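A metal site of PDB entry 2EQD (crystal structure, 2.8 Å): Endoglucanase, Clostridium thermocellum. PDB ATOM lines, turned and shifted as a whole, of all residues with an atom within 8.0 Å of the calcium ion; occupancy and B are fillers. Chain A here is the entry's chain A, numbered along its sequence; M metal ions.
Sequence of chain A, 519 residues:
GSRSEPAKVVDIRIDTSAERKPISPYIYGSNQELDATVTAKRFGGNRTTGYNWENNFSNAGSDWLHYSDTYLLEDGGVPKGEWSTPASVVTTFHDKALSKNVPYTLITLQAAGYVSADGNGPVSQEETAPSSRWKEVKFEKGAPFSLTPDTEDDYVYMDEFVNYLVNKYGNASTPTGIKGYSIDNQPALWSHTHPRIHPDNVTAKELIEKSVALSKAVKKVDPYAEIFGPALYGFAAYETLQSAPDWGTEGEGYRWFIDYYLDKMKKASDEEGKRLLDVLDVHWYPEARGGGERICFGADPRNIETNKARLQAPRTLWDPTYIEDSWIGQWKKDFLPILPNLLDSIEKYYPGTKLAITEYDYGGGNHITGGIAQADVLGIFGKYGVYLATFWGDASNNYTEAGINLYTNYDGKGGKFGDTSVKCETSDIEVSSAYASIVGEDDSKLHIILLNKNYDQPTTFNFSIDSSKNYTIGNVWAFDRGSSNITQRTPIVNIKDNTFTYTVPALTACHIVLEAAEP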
ATOM      1  N   ASN A  52      20.835  22.426  13.645  1.00  0.00           N
ATOM      2  CA  ASN A  52      20.338  22.126  14.983  1.00  0.00           C
ATOM      3  C   ASN A  52      21.516  21.824  15.908  1.00  0.00           C
ATOM      4  O   ASN A  52      22.105  20.755  15.832  1.00  0.00           O
ATOM      5  CB  ASN A  52      19.407  20.908  14.924  1.00  0.00           C
ATOM      6  CG  ASN A  52      18.683  20.662  16.226  1.00  0.00           C
ATOM      7  OD1 ASN A  52      19.015  21.226  17.256  1.00  0.00           O
ATOM      8  ND2 ASN A  52      17.667  19.797  16.180  1.00  0.00           N
ATOM      9  N   TRP A  53      21.836  22.756  16.796  1.00  0.00           N
ATOM     10  CA  TRP A  53      22.962  22.580  17.710  1.00  0.00           C
ATOM     11  C   TRP A  53      22.905  21.366  18.641  1.00  0.00           C
ATOM     12  O   TRP A  53      23.941  20.863  19.060  1.00  0.00           O
ATOM     13  CB  TRP A  53      23.172  23.833  18.563  1.00  0.00           C
ATOM     14  CG  TRP A  53      22.172  24.057  19.644  1.00  0.00           C
ATOM     15  CD1 TRP A  53      20.925  24.585  19.521  1.00  0.00           C
ATOM     16  CD2 TRP A  53      22.381  23.842  21.038  1.00  0.00           C
ATOM     17  NE1 TRP A  53      20.341  24.725  20.755  1.00  0.00           N
ATOM     18  CE2 TRP A  53      21.217  24.280  21.708  1.00  0.00           C
ATOM     19  CE3 TRP A  53      23.443  23.337  21.802  1.00  0.00           C
ATOM     20  CZ2 TRP A  53      21.074  24.220  23.095  1.00  0.00           C
ATOM     21  CZ3 TRP A  53      23.300  23.277  23.190  1.00  0.00           C
ATOM     22  CH2 TRP A  53      22.123  23.711  23.825  1.00  0.00           C
ATOM     23  N   GLU A  54      21.702  20.912  18.968  1.00  0.00           N
ATOM     24  CA  GLU A  54      21.529  19.764  19.855  1.00  0.00           C
ATOM     25  C   GLU A  54      22.029  18.465  19.217  1.00  0.00           C
ATOM     26  O   GLU A  54      22.525  17.588  19.923  1.00  0.00           O
ATOM     27  CB  GLU A  54      20.063  19.581  20.250  1.00  0.00           C
ATOM     28  CG  GLU A  54      19.224  20.862  20.292  1.00  0.00           C
ATOM     29  CD  GLU A  54      17.882  20.663  20.995  1.00  0.00           C
ATOM     30  OE1 GLU A  54      17.214  19.634  20.722  1.00  0.00           O
ATOM     31  OE2 GLU A  54      17.499  21.542  21.807  1.00  0.00           O
ATOM     32  N   ASN A  55      21.906  18.348  17.895  1.00  0.00           N
ATOM     33  CA  ASN A  55      22.332  17.131  17.202  1.00  0.00           C
ATOM     34  C   ASN A  55      23.202  17.331  15.950  1.00  0.00           C
ATOM     35  O   ASN A  55      23.619  16.352  15.323  1.00  0.00           O
ATOM     36  CB  ASN A  55      21.106  16.283  16.820  1.00  0.00           C
ATOM     37  CG  ASN A  55      20.103  17.043  15.975  1.00  0.00           C
ATOM     38  OD1 ASN A  55      20.473  17.827  15.100  1.00  0.00           O
ATOM     39  ND2 ASN A  55      18.820  16.802  16.217  1.00  0.00           N
ATOM     40  N   LYS A 135      12.222  20.497  14.213  1.00  0.00           N
ATOM     41  CA  LYS A 135      12.053  20.886  15.605  1.00  0.00           C
ATOM     42  C   LYS A 135      11.819  22.387  15.469  1.00  0.00           C
ATOM     43  O   LYS A 135      12.401  23.048  14.599  1.00  0.00           O
ATOM     44  CB  LYS A 135      13.332  20.609  16.395  1.00  0.00           C
ATOM     45  CG  LYS A 135      13.693  19.145  16.515  1.00  0.00           C
ATOM     46  CD  LYS A 135      12.511  18.350  17.061  1.00  0.00           C
ATOM     47  CE  LYS A 135      12.819  16.852  17.163  1.00  0.00           C
ATOM     48  NZ  LYS A 135      11.595  16.064  17.493  1.00  0.00           N
ATOM     49  N   GLU A 136      10.931  22.934  16.297  1.00  0.00           N
ATOM     50  CA  GLU A 136      10.647  24.348  16.211  1.00  0.00           C
ATOM     51  C   GLU A 136      11.688  25.178  16.949  1.00  0.00           C
ATOM     52  O   GLU A 136      11.988  24.940  18.122  1.00  0.00           O
ATOM     53  CB  GLU A 136       9.254  24.639  16.759  1.00  0.00           C
ATOM     54  CG  GLU A 136       8.743  26.023  16.415  1.00  0.00           C
ATOM     55  CD  GLU A 136       7.342  26.242  16.926  1.00  0.00           C
ATOM     56  OE1 GLU A 136       6.455  25.436  16.573  1.00  0.00           O
ATOM     57  OE2 GLU A 136       7.126  27.218  17.670  1.00  0.00           O
ATOM     58  N   LYS A 141      14.308  30.241  26.107  1.00  0.00           N
ATOM     59  CA  LYS A 141      13.849  28.979  26.688  1.00  0.00           C
ATOM     60  C   LYS A 141      12.851  29.116  27.822  1.00  0.00           C
ATOM     61  O   LYS A 141      12.158  28.158  28.171  1.00  0.00           O
ATOM     62  CB  LYS A 141      15.044  28.158  27.180  1.00  0.00           C
ATOM     63  CG  LYS A 141      14.645  26.841  27.811  1.00  0.00           C
ATOM     64  CD  LYS A 141      15.847  25.976  28.151  1.00  0.00           C
ATOM     65  CE  LYS A 141      15.404  24.622  28.706  1.00  0.00           C
ATOM     66  NZ  LYS A 141      16.513  23.622  28.780  1.00  0.00           N
ATOM     67  N   THR A 148      23.060  19.779  28.163  1.00  0.00           N
ATOM     68  CA  THR A 148      22.649  18.483  27.609  1.00  0.00           C
ATOM     69  C   THR A 148      21.250  18.686  27.047  1.00  0.00           C
ATOM     70  O   THR A 148      20.271  18.168  27.579  1.00  0.00           O
ATOM     71  CB  THR A 148      22.584  17.368  28.687  1.00  0.00           C
ATOM     72  OG1 THR A 148      22.268  17.963  29.958  1.00  0.00           O
ATOM     73  CG2 THR A 148      23.896  16.602  28.760  1.00  0.00           C
ATOM     74  N   PRO A 149      21.139  19.441  25.948  1.00  0.00           N
ATOM     75  CA  PRO A 149      19.835  19.704  25.352  1.00  0.00           C
ATOM     76  C   PRO A 149      19.028  18.429  25.159  1.00  0.00           C
ATOM     77  O   PRO A 149      19.577  17.322  25.050  1.00  0.00           O
ATOM     78  CB  PRO A 149      20.195  20.377  24.033  1.00  0.00           C
ATOM     79  CG  PRO A 149      21.460  19.705  23.666  1.00  0.00           C
ATOM     80  CD  PRO A 149      22.219  19.720  24.979  1.00  0.00           C
ATOM     81  N   ASP A 150      17.711  18.608  25.136  1.00  0.00           N
ATOM     82  CA  ASP A 150      16.798  17.490  24.959  1.00  0.00           C
ATOM     83  C   ASP A 150      16.494  17.336  23.480  1.00  0.00           C
ATOM     84  O   ASP A 150      15.688  18.063  22.916  1.00  0.00           O
ATOM     85  CB  ASP A 150      15.502  17.754  25.732  1.00  0.00           C
ATOM     86  CG  ASP A 150      14.666  16.509  25.898  1.00  0.00           C
ATOM     87  OD1 ASP A 150      14.915  15.509  25.186  1.00  0.00           O
ATOM     88  OD2 ASP A 150      13.753  16.541  26.751  1.00  0.00           O
ATOM     89  N   THR A 151      17.157  16.371  22.833  1.00  0.00           N
ATOM     90  CA  THR A 151      16.937  16.141  21.416  1.00  0.00           C
ATOM     91  C   THR A 151      15.536  15.595  21.174  1.00  0.00           C
ATOM     92  O   THR A 151      15.056  15.569  20.042  1.00  0.00           O
ATOM     93  CB  THR A 151      17.935  15.112  20.866  1.00  0.00           C
ATOM     94  OG1 THR A 151      17.557  13.799  21.317  1.00  0.00           O
ATOM     95  CG2 THR A 151      19.334  15.423  21.370  1.00  0.00           C
ATOM     96  N   GLU A 152      14.875  15.155  22.243  1.00  0.00           N
ATOM     97  CA  GLU A 152      13.556  14.577  22.113  1.00  0.00           C
ATOM     98  C   GLU A 152      12.386  15.535  22.121  1.00  0.00           C
ATOM     99  O   GLU A 152      11.336  15.209  21.580  1.00  0.00           O
ATOM    100  CB  GLU A 152      13.349  13.526  23.192  1.00  0.00           C
ATOM    101  CG  GLU A 152      14.267  12.344  23.041  1.00  0.00           C
ATOM    102  CD  GLU A 152      13.984  11.269  24.068  1.00  0.00           C
ATOM    103  OE1 GLU A 152      14.008  11.595  25.278  1.00  0.00           O
ATOM    104  OE2 GLU A 152      13.741  10.112  23.669  1.00  0.00           O
ATOM    105  N   ASP A 153      12.544  16.713  22.720  1.00  0.00           N
ATOM    106  CA  ASP A 153      11.425  17.651  22.709  1.00  0.00           C
ATOM    107  C   ASP A 153      11.187  18.156  21.286  1.00  0.00           C
ATOM    108  O   ASP A 153      11.891  17.776  20.345  1.00  0.00           O
ATOM    109  CB  ASP A 153      11.657  18.831  23.664  1.00  0.00           C
ATOM    110  CG  ASP A 153      12.978  19.539  23.408  1.00  0.00           C
ATOM    111  OD1 ASP A 153      13.330  19.754  22.229  1.00  0.00           O
ATOM    112  OD2 ASP A 153      13.640  19.902  24.402  1.00  0.00           O
ATOM    113  N   ASP A 154      10.191  19.017  21.133  1.00  0.00           N
ATOM    114  CA  ASP A 154       9.887  19.557  19.830  1.00  0.00           C
ATOM    115  C   ASP A 154      10.510  20.926  19.644  1.00  0.00           C
ATOM    116  O   ASP A 154      10.140  21.670  18.738  1.00  0.00           O
ATOM    117  CB  ASP A 154       8.370  19.631  19.642  1.00  0.00           C
ATOM    118  CG  ASP A 154       7.698  18.282  19.719  1.00  0.00           C
ATOM    119  OD1 ASP A 154       8.155  17.342  19.034  1.00  0.00           O
ATOM    120  OD2 ASP A 154       6.703  18.164  20.474  1.00  0.00           O
ATOM    121  N   TYR A 155      11.483  21.268  20.483  1.00  0.00           N
ATOM    122  CA  TYR A 155      12.111  22.570  20.387  1.00  0.00           C
ATOM    123  C   TYR A 155      13.629  22.624  20.473  1.00  0.00           C
ATOM    124  O   TYR A 155      14.280  21.679  20.928  1.00  0.00           O
ATOM    125  CB  TYR A 155      11.535  23.490  21.465  1.00  0.00           C
ATOM    126  CG  TYR A 155      10.037  23.599  21.412  1.00  0.00           C
ATOM    127  CD1 TYR A 155       9.397  24.073  20.270  1.00  0.00           C
ATOM    128  CD2 TYR A 155       9.254  23.270  22.510  1.00  0.00           C
ATOM    129  CE1 TYR A 155       8.020  24.222  20.222  1.00  0.00           C
ATOM    130  CE2 TYR A 155       7.882  23.406  22.483  1.00  0.00           C
ATOM    131  CZ  TYR A 155       7.265  23.883  21.332  1.00  0.00           C
ATOM    132  OH  TYR A 155       5.895  24.061  21.306  1.00  0.00           O
ATOM    133  N   VAL A 156      14.159  23.741  20.015  1.00  0.00           N
ATOM    134  CA  VAL A 156      15.589  24.043  20.026  1.00  0.00           C
ATOM    135  C   VAL A 156      15.635  25.521  20.426  1.00  0.00           C
ATOM    136  O   VAL A 156      14.998  26.366  19.802  1.00  0.00           O
ATOM    137  CB  VAL A 156      16.229  23.850  18.643  1.00  0.00           C
ATOM    138  CG1 VAL A 156      17.582  24.502  18.609  1.00  0.00           C
ATOM    139  CG2 VAL A 156      16.362  22.378  18.342  1.00  0.00           C
ATOM    140  N   TYR A 157      16.375  25.811  21.489  1.00  0.00           N
ATOM    141  CA  TYR A 157      16.465  27.176  21.994  1.00  0.00           C
ATOM    142  C   TYR A 157      17.756  27.864  21.577  1.00  0.00           C
ATOM    143  O   TYR A 157      18.856  27.327  21.782  1.00  0.00           O
ATOM    144  CB  TYR A 157      16.300  27.145  23.513  1.00  0.00           C
ATOM    145  CG  TYR A 157      14.966  26.580  23.938  1.00  0.00           C
ATOM    146  CD1 TYR A 157      13.824  27.388  23.960  1.00  0.00           C
ATOM    147  CD2 TYR A 157      14.820  25.221  24.219  1.00  0.00           C
ATOM    148  CE1 TYR A 157      12.563  26.849  24.253  1.00  0.00           C
ATOM    149  CE2 TYR A 157      13.574  24.666  24.503  1.00  0.00           C
ATOM    150  CZ  TYR A 157      12.442  25.482  24.517  1.00  0.00           C
ATOM    151  OH  TYR A 157      11.203  24.935  24.765  1.00  0.00           O
ATOM    152  N   GLU A 160      19.776  29.295  24.591  1.00  0.00           N
ATOM    153  CA  GLU A 160      20.420  28.201  25.318  1.00  0.00           C
ATOM    154  C   GLU A 160      21.652  27.748  24.536  1.00  0.00           C
ATOM    155  O   GLU A 160      22.634  27.264  25.102  1.00  0.00           O
ATOM    156  CB  GLU A 160      19.460  27.024  25.497  1.00  0.00           C
ATOM    157  CG  GLU A 160      20.084  25.884  26.275  1.00  0.00           C
ATOM    158  CD  GLU A 160      19.217  24.630  26.315  1.00  0.00           C
ATOM    159  OE1 GLU A 160      18.728  24.223  25.234  1.00  0.00           O
ATOM    160  OE2 GLU A 160      19.031  24.053  27.403  1.00  0.00           O
HETATM  161 CA    CA M   1      15.450  20.276  22.075  1.00  0.00          CA
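O of Asp 153 is in hydrogen-bond range of NZ of Lys 135, 3.3 Å away.
The side-chain amide oxygen (OD1) of Asn 52 lies close to the backbone NH (N) of Glu 54, 3.2 Å away.
OD1 of Asp 150 lies within hydrogen-bond range of N of Glu 152 (3.0 Å).
Four residues have an atom within 4 Å of the calcium ion: Glu 54, Asp 150, Asp 153 and Tyr 155.
The calcium ion is bound by O of Tyr 155 (2.2 Å), OD1 of Asp 153 (2.2 Å), OE1 of Glu 54 (2.3 Å), O of Asp 150 (2.4 Å) and OE2 of Glu 54 (2.4 Å).
The calcium ion has five donor atoms within binding distance.
Slightly farther from the calcium ion lies OD2 of Asp 153 (3.0 Å).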
